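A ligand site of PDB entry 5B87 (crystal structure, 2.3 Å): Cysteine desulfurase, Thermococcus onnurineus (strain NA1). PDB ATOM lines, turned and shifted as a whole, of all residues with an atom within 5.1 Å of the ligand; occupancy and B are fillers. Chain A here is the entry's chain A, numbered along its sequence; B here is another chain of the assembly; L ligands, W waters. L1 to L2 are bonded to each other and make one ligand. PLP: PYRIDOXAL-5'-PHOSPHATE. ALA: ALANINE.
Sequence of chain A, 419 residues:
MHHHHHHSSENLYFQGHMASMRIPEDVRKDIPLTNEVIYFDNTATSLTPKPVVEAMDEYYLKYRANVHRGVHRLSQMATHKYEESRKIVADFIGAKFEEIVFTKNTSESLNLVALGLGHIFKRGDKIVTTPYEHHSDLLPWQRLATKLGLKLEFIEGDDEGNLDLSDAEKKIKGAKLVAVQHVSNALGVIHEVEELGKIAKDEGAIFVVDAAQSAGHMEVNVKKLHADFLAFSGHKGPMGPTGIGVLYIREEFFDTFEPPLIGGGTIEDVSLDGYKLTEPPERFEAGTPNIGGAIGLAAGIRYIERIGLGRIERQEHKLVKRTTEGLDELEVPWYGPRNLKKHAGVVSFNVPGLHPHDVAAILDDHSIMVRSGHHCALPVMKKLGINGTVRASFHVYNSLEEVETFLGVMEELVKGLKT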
ATOM      1  N   THR A  43     -20.445  19.312  11.819  1.00  0.00           N
ATOM      2  CA  THR A  43     -20.584  19.978  13.104  1.00  0.00           C
ATOM      3  C   THR A  43     -22.057  20.219  13.389  1.00  0.00           C
ATOM      4  O   THR A  43     -22.436  20.311  14.568  1.00  0.00           O
ATOM      5  CB  THR A  43     -19.613  21.223  13.341  1.00  0.00           C
ATOM      6  OG1 THR A  43     -20.271  22.509  13.470  1.00  0.00           O
ATOM      7  CG2 THR A  43     -18.585  21.304  12.341  1.00  0.00           C
ATOM      8  N   ALA A  44     -22.923  20.280  12.346  1.00  0.00           N
ATOM      9  CA  ALA A  44     -24.350  20.550  12.612  1.00  0.00           C
ATOM     10  C   ALA A  44     -24.919  19.290  13.151  1.00  0.00           C
ATOM     11  O   ALA A  44     -25.652  19.305  14.132  1.00  0.00           O
ATOM     12  CB  ALA A  44     -25.084  20.945  11.334  1.00  0.00           C
ATOM     13  N   ASN A 105     -30.493  17.170  24.432  1.00  0.00           N
ATOM     14  CA  ASN A 105     -29.330  17.643  23.751  1.00  0.00           C
ATOM     15  C   ASN A 105     -28.432  18.434  24.744  1.00  0.00           C
ATOM     16  O   ASN A 105     -28.786  18.573  25.963  1.00  0.00           O
ATOM     17  CB  ASN A 105     -29.771  18.534  22.600  1.00  0.00           C
ATOM     18  CG  ASN A 105     -30.685  19.622  23.038  1.00  0.00           C
ATOM     19  OD1 ASN A 105     -30.556  20.122  24.139  1.00  0.00           O
ATOM     20  ND2 ASN A 105     -31.603  20.024  22.191  1.00  0.00           N
ATOM     21  N   THR A 106     -27.311  18.909  24.181  1.00  0.00           N
ATOM     22  CA  THR A 106     -26.300  19.651  24.889  1.00  0.00           C
ATOM     23  C   THR A 106     -26.974  20.893  25.429  1.00  0.00           C
ATOM     24  O   THR A 106     -26.723  21.259  26.561  1.00  0.00           O
ATOM     25  CB  THR A 106     -25.097  20.033  23.954  1.00  0.00           C
ATOM     26  OG1 THR A 106     -24.297  18.902  23.614  1.00  0.00           O
ATOM     27  CG2 THR A 106     -24.147  21.023  24.675  1.00  0.00           C
ATOM     28  N   SER A 107     -27.820  21.543  24.632  1.00  0.00           N
ATOM     29  CA  SER A 107     -28.441  22.750  25.085  1.00  0.00           C
ATOM     30  C   SER A 107     -29.291  22.512  26.347  1.00  0.00           C
ATOM     31  O   SER A 107     -29.250  23.302  27.294  1.00  0.00           O
ATOM     32  CB  SER A 107     -29.248  23.384  23.964  1.00  0.00           C
ATOM     33  OG  SER A 107     -28.499  23.479  22.777  1.00  0.00           O
ATOM     34  N   LEU A 110     -26.786  21.895  29.418  1.00  0.00           N
ATOM     35  CA  LEU A 110     -26.220  23.147  29.879  1.00  0.00           C
ATOM     36  C   LEU A 110     -27.208  23.971  30.680  1.00  0.00           C
ATOM     37  O   LEU A 110     -26.913  24.400  31.756  1.00  0.00           O
ATOM     38  CB  LEU A 110     -25.650  23.902  28.693  1.00  0.00           C
ATOM     39  CG  LEU A 110     -24.184  23.868  28.318  1.00  0.00           C
ATOM     40  CD1 LEU A 110     -23.267  22.980  29.099  1.00  0.00           C
ATOM     41  CD2 LEU A 110     -23.889  23.905  26.854  1.00  0.00           C
ATOM     42  N   HIS A 134     -20.935  29.049  21.946  1.00  0.00           N
ATOM     43  CA  HIS A 134     -22.119  28.787  21.203  1.00  0.00           C
ATOM     44  C   HIS A 134     -23.193  29.361  22.115  1.00  0.00           C
ATOM     45  O   HIS A 134     -23.052  29.309  23.293  1.00  0.00           O
ATOM     46  CB  HIS A 134     -22.270  27.269  21.069  1.00  0.00           C
ATOM     47  CG  HIS A 134     -23.571  26.837  20.502  1.00  0.00           C
ATOM     48  ND1 HIS A 134     -23.739  26.527  19.172  1.00  0.00           N
ATOM     49  CD2 HIS A 134     -24.781  26.647  21.073  1.00  0.00           C
ATOM     50  CE1 HIS A 134     -24.989  26.183  18.960  1.00  0.00           C
ATOM     51  NE2 HIS A 134     -25.633  26.233  20.098  1.00  0.00           N
ATOM     52  N   SER A 136     -25.804  28.299  23.419  1.00  0.00           N
ATOM     53  CA  SER A 136     -26.236  27.417  24.461  1.00  0.00           C
ATOM     54  C   SER A 136     -25.320  27.408  25.656  1.00  0.00           C
ATOM     55  O   SER A 136     -25.742  27.039  26.706  1.00  0.00           O
ATOM     56  CB  SER A 136     -26.421  26.009  23.936  1.00  0.00           C
ATOM     57  OG  SER A 136     -27.510  25.941  23.093  1.00  0.00           O
ATOM     58  N   GLN A 181     -16.070  25.845  26.260  1.00  0.00           N
ATOM     59  CA  GLN A 181     -16.336  24.892  25.235  1.00  0.00           C
ATOM     60  C   GLN A 181     -15.045  24.162  24.991  1.00  0.00           C
ATOM     61  O   GLN A 181     -14.012  24.732  25.121  1.00  0.00           O
ATOM     62  CB  GLN A 181     -16.807  25.578  23.972  1.00  0.00           C
ATOM     63  CG  GLN A 181     -15.721  26.246  23.167  1.00  0.00           C
ATOM     64  CD  GLN A 181     -16.234  27.225  22.150  1.00  0.00           C
ATOM     65  OE1 GLN A 181     -17.397  27.271  21.858  1.00  0.00           O
ATOM     66  NE2 GLN A 181     -15.347  28.004  21.612  1.00  0.00           N
ATOM     67  N   VAL A 183     -14.351  22.489  22.033  1.00  0.00           N
ATOM     68  CA  VAL A 183     -14.022  22.945  20.700  1.00  0.00           C
ATOM     69  C   VAL A 183     -15.105  23.903  20.198  1.00  0.00           C
ATOM     70  O   VAL A 183     -16.242  23.729  20.498  1.00  0.00           O
ATOM     71  CB  VAL A 183     -13.616  21.835  19.707  1.00  0.00           C
ATOM     72  CG1 VAL A 183     -13.887  20.478  20.237  1.00  0.00           C
ATOM     73  CG2 VAL A 183     -14.103  22.039  18.301  1.00  0.00           C
ATOM     74  N   ASN A 185     -17.537  25.538  17.533  1.00  0.00           N
ATOM     75  CA  ASN A 185     -18.264  25.027  16.359  1.00  0.00           C
ATOM     76  C   ASN A 185     -18.149  26.006  15.187  1.00  0.00           C
ATOM     77  O   ASN A 185     -18.570  25.673  14.070  1.00  0.00           O
ATOM     78  CB  ASN A 185     -19.721  24.842  16.718  1.00  0.00           C
ATOM     79  CG  ASN A 185     -20.337  26.149  17.258  1.00  0.00           C
ATOM     80  OD1 ASN A 185     -19.815  26.756  18.215  1.00  0.00           O
ATOM     81  ND2 ASN A 185     -21.380  26.592  16.625  1.00  0.00           N
ATOM     82  N   ASP A 210     -18.465  22.146  27.853  1.00  0.00           N
ATOM     83  CA  ASP A 210     -19.346  21.937  26.700  1.00  0.00           C
ATOM     84  C   ASP A 210     -18.554  21.177  25.675  1.00  0.00           C
ATOM     85  O   ASP A 210     -17.762  21.753  24.981  1.00  0.00           O
ATOM     86  CB  ASP A 210     -19.852  23.289  26.132  1.00  0.00           C
ATOM     87  CG  ASP A 210     -20.516  23.155  24.748  1.00  0.00           C
ATOM     88  OD1 ASP A 210     -20.723  22.009  24.241  1.00  0.00           O
ATOM     89  OD2 ASP A 210     -20.814  24.235  24.173  1.00  0.00           O
ATOM     90  N   ALA A 212     -19.753  19.450  23.003  1.00  0.00           N
ATOM     91  CA  ALA A 212     -20.604  19.198  21.837  1.00  0.00           C
ATOM     92  C   ALA A 212     -19.865  18.880  20.555  1.00  0.00           C
ATOM     93  O   ALA A 212     -20.292  18.076  19.786  1.00  0.00           O
ATOM     94  CB  ALA A 212     -21.557  20.374  21.600  1.00  0.00           C
ATOM     95  N   GLN A 213     -18.745  19.530  20.367  1.00  0.00           N
ATOM     96  CA  GLN A 213     -17.937  19.358  19.198  1.00  0.00           C
ATOM     97  C   GLN A 213     -16.721  18.484  19.379  1.00  0.00           C
ATOM     98  O   GLN A 213     -16.032  18.260  18.447  1.00  0.00           O
ATOM     99  CB  GLN A 213     -17.525  20.700  18.644  1.00  0.00           C
ATOM    100  CG  GLN A 213     -18.601  21.391  17.865  1.00  0.00           C
ATOM    101  CD  GLN A 213     -19.261  20.487  16.845  1.00  0.00           C
ATOM    102  OE1 GLN A 213     -18.616  19.708  16.178  1.00  0.00           O
ATOM    103  NE2 GLN A 213     -20.553  20.602  16.743  1.00  0.00           N
ATOM    104  N   SER A 233     -23.872  15.904  22.833  1.00  0.00           N
ATOM    105  CA  SER A 233     -25.024  15.603  22.028  1.00  0.00           C
ATOM    106  C   SER A 233     -24.792  14.372  21.217  1.00  0.00           C
ATOM    107  O   SER A 233     -23.883  14.289  20.409  1.00  0.00           O
ATOM    108  CB  SER A 233     -25.300  16.780  21.109  1.00  0.00           C
ATOM    109  OG  SER A 233     -25.956  17.841  21.756  1.00  0.00           O
ATOM    110  N   HIS A 235     -26.240  13.202  18.578  1.00  0.00           N
ATOM    111  CA  HIS A 235     -26.376  13.381  17.142  1.00  0.00           C
ATOM    112  C   HIS A 235     -25.219  13.956  16.367  1.00  0.00           C
ATOM    113  O   HIS A 235     -25.260  13.985  15.175  1.00  0.00           O
ATOM    114  CB  HIS A 235     -27.664  14.148  16.828  1.00  0.00           C
ATOM    115  CG  HIS A 235     -27.577  15.604  17.134  1.00  0.00           C
ATOM    116  ND1 HIS A 235     -27.207  16.527  16.200  1.00  0.00           N
ATOM    117  CD2 HIS A 235     -27.730  16.269  18.288  1.00  0.00           C
ATOM    118  CE1 HIS A 235     -27.190  17.712  16.749  1.00  0.00           C
ATOM    119  NE2 HIS A 235     -27.512  17.589  18.020  1.00  0.00           N
ATOM    120  N   LYS A 236     -24.238  14.352  17.045  1.00  0.00           N
ATOM    121  CA  LYS A 236     -23.068  14.903  16.416  1.00  0.00           C
ATOM    122  C   LYS A 236     -21.973  13.863  16.219  1.00  0.00           C
ATOM    123  O   LYS A 236     -22.191  12.890  15.559  1.00  0.00           O
ATOM    124  CB  LYS A 236     -22.620  16.166  17.151  1.00  0.00           C
ATOM    125  CG  LYS A 236     -23.586  17.293  17.093  1.00  0.00           C
ATOM    126  CD  LYS A 236     -23.436  18.517  17.975  1.00  0.00           C
ATOM    127  CE  LYS A 236     -24.424  19.725  17.723  1.00  0.00           C
ATOM    128  NZ  LYS A 236     -23.737  20.995  18.021  1.00  0.00           N
ATOM    129  N   ARG A 371     -22.480  24.427   5.670  1.00  0.00           N
ATOM    130  CA  ARG A 371     -23.325  25.307   6.384  1.00  0.00           C
ATOM    131  C   ARG A 371     -22.814  26.735   6.204  1.00  0.00           C
ATOM    132  O   ARG A 371     -21.606  26.935   6.069  1.00  0.00           O
ATOM    133  CB  ARG A 371     -23.293  24.976   7.855  1.00  0.00           C
ATOM    134  CG  ARG A 371     -24.556  25.459   8.565  1.00  0.00           C
ATOM    135  CD  ARG A 371     -25.552  24.321   8.806  1.00  0.00           C
ATOM    136  NE  ARG A 371     -26.918  24.784   8.993  1.00  0.00           N
ATOM    137  CZ  ARG A 371     -27.976  23.993   9.160  1.00  0.00           C
ATOM    138  NH1 ARG A 371     -27.860  22.655   9.133  1.00  0.00           N
ATOM    139  NH2 ARG A 371     -29.178  24.562   9.331  1.00  0.00           N
ATOM    140  N   HIS A 375     -23.712  30.336  12.755  1.00  0.00           N
ATOM    141  CA  HIS A 375     -23.558  29.091  13.501  1.00  0.00           C
ATOM    142  C   HIS A 375     -23.880  29.159  14.948  1.00  0.00           C
ATOM    143  O   HIS A 375     -23.275  28.505  15.741  1.00  0.00           O
ATOM    144  CB  HIS A 375     -22.181  28.503  13.269  1.00  0.00           C
ATOM    145  CG  HIS A 375     -21.678  28.686  11.875  1.00  0.00           C
ATOM    146  ND1 HIS A 375     -22.323  28.157  10.791  1.00  0.00           N
ATOM    147  CD2 HIS A 375     -20.615  29.346  11.399  1.00  0.00           C
ATOM    148  CE1 HIS A 375     -21.677  28.504   9.697  1.00  0.00           C
ATOM    149  NE2 HIS A 375     -20.625  29.208  10.045  1.00  0.00           N
ATOM    150  N   ARG A 391     -19.103  27.011   6.386  1.00  0.00           N
ATOM    151  CA  ARG A 391     -18.444  26.030   7.189  1.00  0.00           C
ATOM    152  C   ARG A 391     -18.472  24.613   6.682  1.00  0.00           C
ATOM    153  O   ARG A 391     -19.481  24.017   6.589  1.00  0.00           O
ATOM    154  CB  ARG A 391     -19.002  26.117   8.587  1.00  0.00           C
ATOM    155  CG  ARG A 391     -18.343  25.249   9.614  1.00  0.00           C
ATOM    156  CD  ARG A 391     -19.132  25.275  10.876  1.00  0.00           C
ATOM    157  NE  ARG A 391     -20.328  24.494  10.759  1.00  0.00           N
ATOM    158  CZ  ARG A 391     -21.320  24.502  11.618  1.00  0.00           C
ATOM    159  NH1 ARG A 391     -21.258  25.227  12.703  1.00  0.00           N
ATOM    160  NH2 ARG A 391     -22.371  23.771  11.398  1.00  0.00           N
ATOM    161  N   ASN B  66     -29.478  18.591  10.085  1.00  0.00           N
ATOM    162  CA  ASN B  66     -30.097  19.416  11.121  1.00  0.00           C
ATOM    163  C   ASN B  66     -31.111  20.361  10.414  1.00  0.00           C
ATOM    164  O   ASN B  66     -31.087  20.503   9.199  1.00  0.00           O
ATOM    165  CB  ASN B  66     -29.045  20.221  11.877  1.00  0.00           C
ATOM    166  CG  ASN B  66     -29.441  20.524  13.278  1.00  0.00           C
ATOM    167  OD1 ASN B  66     -30.624  20.719  13.566  1.00  0.00           O
ATOM    168  ND2 ASN B  66     -28.464  20.544  14.203  1.00  0.00           N
ATOM    169  N   HIS B  68     -33.206  24.333  11.131  1.00  0.00           N
ATOM    170  CA  HIS B  68     -32.924  25.759  11.040  1.00  0.00           C
ATOM    171  C   HIS B  68     -32.620  26.210   9.595  1.00  0.00           C
ATOM    172  O   HIS B  68     -31.727  26.978   9.377  1.00  0.00           O
ATOM    173  CB  HIS B  68     -31.827  26.309  11.994  1.00  0.00           C
ATOM    174  CG  HIS B  68     -31.394  25.387  13.112  1.00  0.00           C
ATOM    175  ND1 HIS B  68     -32.270  24.818  14.006  1.00  0.00           N
ATOM    176  CD2 HIS B  68     -30.157  25.038  13.538  1.00  0.00           C
ATOM    177  CE1 HIS B  68     -31.598  24.114  14.899  1.00  0.00           C
ATOM    178  NE2 HIS B  68     -30.312  24.232  14.641  1.00  0.00           N
ATOM    179  N   ALA B 286     -34.940  24.947  22.838  1.00  0.00           N
ATOM    180  CA  ALA B 286     -33.503  25.131  22.923  1.00  0.00           C
ATOM    181  C   ALA B 286     -32.664  24.015  22.296  1.00  0.00           C
ATOM    182  O   ALA B 286     -32.711  22.889  22.781  1.00  0.00           O
ATOM    183  CB  ALA B 286     -33.110  25.319  24.371  1.00  0.00           C
ATOM    184  N   GLY B 287     -31.822  24.366  21.301  1.00  0.00           N
ATOM    185  CA  GLY B 287     -30.895  23.467  20.676  1.00  0.00           C
ATOM    186  C   GLY B 287     -31.518  22.526  19.654  1.00  0.00           C
ATOM    187  O   GLY B 287     -32.678  22.606  19.386  1.00  0.00           O
ATOM    188  N   THR B 288     -30.722  21.668  19.032  1.00  0.00           N
ATOM    189  CA  THR B 288     -31.192  20.715  18.042  1.00  0.00           C
ATOM    190  C   THR B 288     -32.355  19.906  18.577  1.00  0.00           C
ATOM    191  O   THR B 288     -32.246  19.210  19.597  1.00  0.00           O
ATOM    192  CB  THR B 288     -30.042  19.763  17.589  1.00  0.00           C
ATOM    193  OG1 THR B 288     -28.965  20.591  17.107  1.00  0.00           O
ATOM    194  CG2 THR B 288     -30.490  18.802  16.505  1.00  0.00           C
HETATM  195  N1  PLP L   1     -22.164  23.777  21.853  1.00  0.00           N
HETATM  196  C2  PLP L   1     -21.574  23.577  20.680  1.00  0.00           C
HETATM  197  C2A PLP L   1     -20.086  23.918  20.705  1.00  0.00           C
HETATM  198  C3  PLP L   1     -22.245  23.089  19.502  1.00  0.00           C
HETATM  199  O3  PLP L   1     -21.665  22.875  18.204  1.00  0.00           O
HETATM  200  C4  PLP L   1     -23.564  22.804  19.627  1.00  0.00           C
HETATM  201  C4A PLP L   1     -24.302  22.320  18.294  1.00  0.00           C
HETATM  202  C5  PLP L   1     -24.207  23.056  20.832  1.00  0.00           C
HETATM  203  C6  PLP L   1     -23.469  23.484  21.927  1.00  0.00           C
HETATM  204  C5A PLP L   1     -25.655  22.733  21.015  1.00  0.00           C
HETATM  205  O4P PLP L   1     -25.798  21.288  20.878  1.00  0.00           O
HETATM  206  P   PLP L   1     -27.322  20.794  20.461  1.00  0.00           P
HETATM  207  O1P PLP L   1     -27.309  19.362  20.162  1.00  0.00           O
HETATM  208  O2P PLP L   1     -28.127  21.229  21.593  1.00  0.00           O
HETATM  209  O3P PLP L   1     -27.998  21.589  19.367  1.00  0.00           O
HETATM  210  N   ALA L   2     -24.069  23.205  17.094  1.00  0.00           N
HETATM  211  CA  ALA L   2     -24.637  22.839  15.770  1.00  0.00           C
HETATM  212  C   ALA L   2     -23.992  23.762  14.690  1.00  0.00           C
HETATM  213  O   ALA L   2     -22.882  24.489  15.109  1.00  0.00           O
HETATM  214  CB  ALA L   2     -26.125  22.841  15.691  1.00  0.00           C
HETATM  215  OXT ALA L   2     -24.434  23.871  13.622  1.00  0.00           O
HETATM  216  O   HOH W   1     -28.125  24.425  18.640  1.00  0.00           O
HETATM  217  O   HOH W   2     -24.846  26.264  11.324  1.00  0.00           O
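An oxygen (O) of ALA L2 is in salt-bridge range of the guanidinium group of Arg 391, at 3.0 Å. The side-chain carboxylate (OD2) of Asp 210 sits at hydrogen-bond distance from a nitrogen (N1) of PLP L1 (2.7 Å). A ring nitrogen (NE2) of His 235 sits at hydrogen-bond distance from an oxygen (O1P) of PLP L1. The side-chain amide nitrogen (NE2) of Gln 213 is in hydrogen-bond range of an oxygen (O3) of PLP L1 (2.9 Å). ND2 of Asn 185 is in hydrogen-bond range of O of ALA L2, 3.0 Å away. N of Ser 107 sits at hydrogen-bond distance from O2P of PLP L1 (3.1 Å). The backbone NH (N) of Thr 288 of chain B is in hydrogen-bond range of an oxygen (O3P) of PLP L1, at 2.7 Å. The side-chain hydroxyl (OG) of Ser 233 is in hydrogen-bond range of an oxygen (O1P) of PLP L1 (2.6 Å). The side-chain amino group (NZ) of Lys 236 is bonded to a carbon (C4A) of PLP L1, 1.5 Å away. OG1 of Thr 288 of chain B lies within hydrogen-bond range of O3P of PLP L1 (2.7 Å). An oxygen (O2P) of PLP L1 is in hydrogen-bond range of the side-chain hydroxyl (OG) of Ser 107.
The backbone carbonyl oxygen (O) of His 375 is in hydrogen-bond range of the side-chain amide nitrogen (ND2) of Asn 185. N of Ser 107 is in hydrogen-bond range of OD1 of Asn 105, 3.1 Å away. The side-chain amide nitrogen (ND2) of Asn 66 of chain B is in hydrogen-bond range of the backbone carbonyl oxygen (O) of Ala 44 (3.1 Å). ND2 of Asn 185 lies within hydrogen-bond range of ND1 of His 134 (3.5 Å). The backbone carbonyl oxygen (O) of Thr 43 is in hydrogen-bond range of the side-chain amide nitrogen (NE2) of Gln 213 (2.9 Å). OG1 of Thr 288 of chain B lies close to NE2 of His 235. The side-chain amide nitrogen (NE2) of Gln 213 sits close to the side-chain amino group (NZ) of Lys 236 (3.5 Å). N of Arg 391 sits at hydrogen-bond distance from O of Arg 371.
Residues that only touch the ligand: Thr 43 (3.6 Å), Ala 44 (3.5 Å), Asn 105 (3.3 Å), Thr 106 (3.4 Å), His 134 (3.5 Å), Val 183 (3.9 Å), Ala 212 (3.3 Å), Asn 66 of chain B (3.6 Å) and Gly 287 of chain B (3.7 Å). Hydrophobic or aromatic side chains within 4 Å of the ligand: Ala 44, His 134, Ala 212 and His 235. Along chain A the residues within 4 Å of the ligand span positions 43 to 391. The nearest printed residue that does not touch the ligand is His 375 (4.1 Å).
Water W1 lies within hydrogen-bond range of an oxygen (O3P) of PLP L1 (2.9 Å) and a ring nitrogen (NE2) of His 134 (3.4 Å). Water W2 lies within hydrogen-bond range of ND1 of His 375 (3.2 Å), OXT of ALA L2 (3.3 Å) and NE of Arg 371 (3.5 Å).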
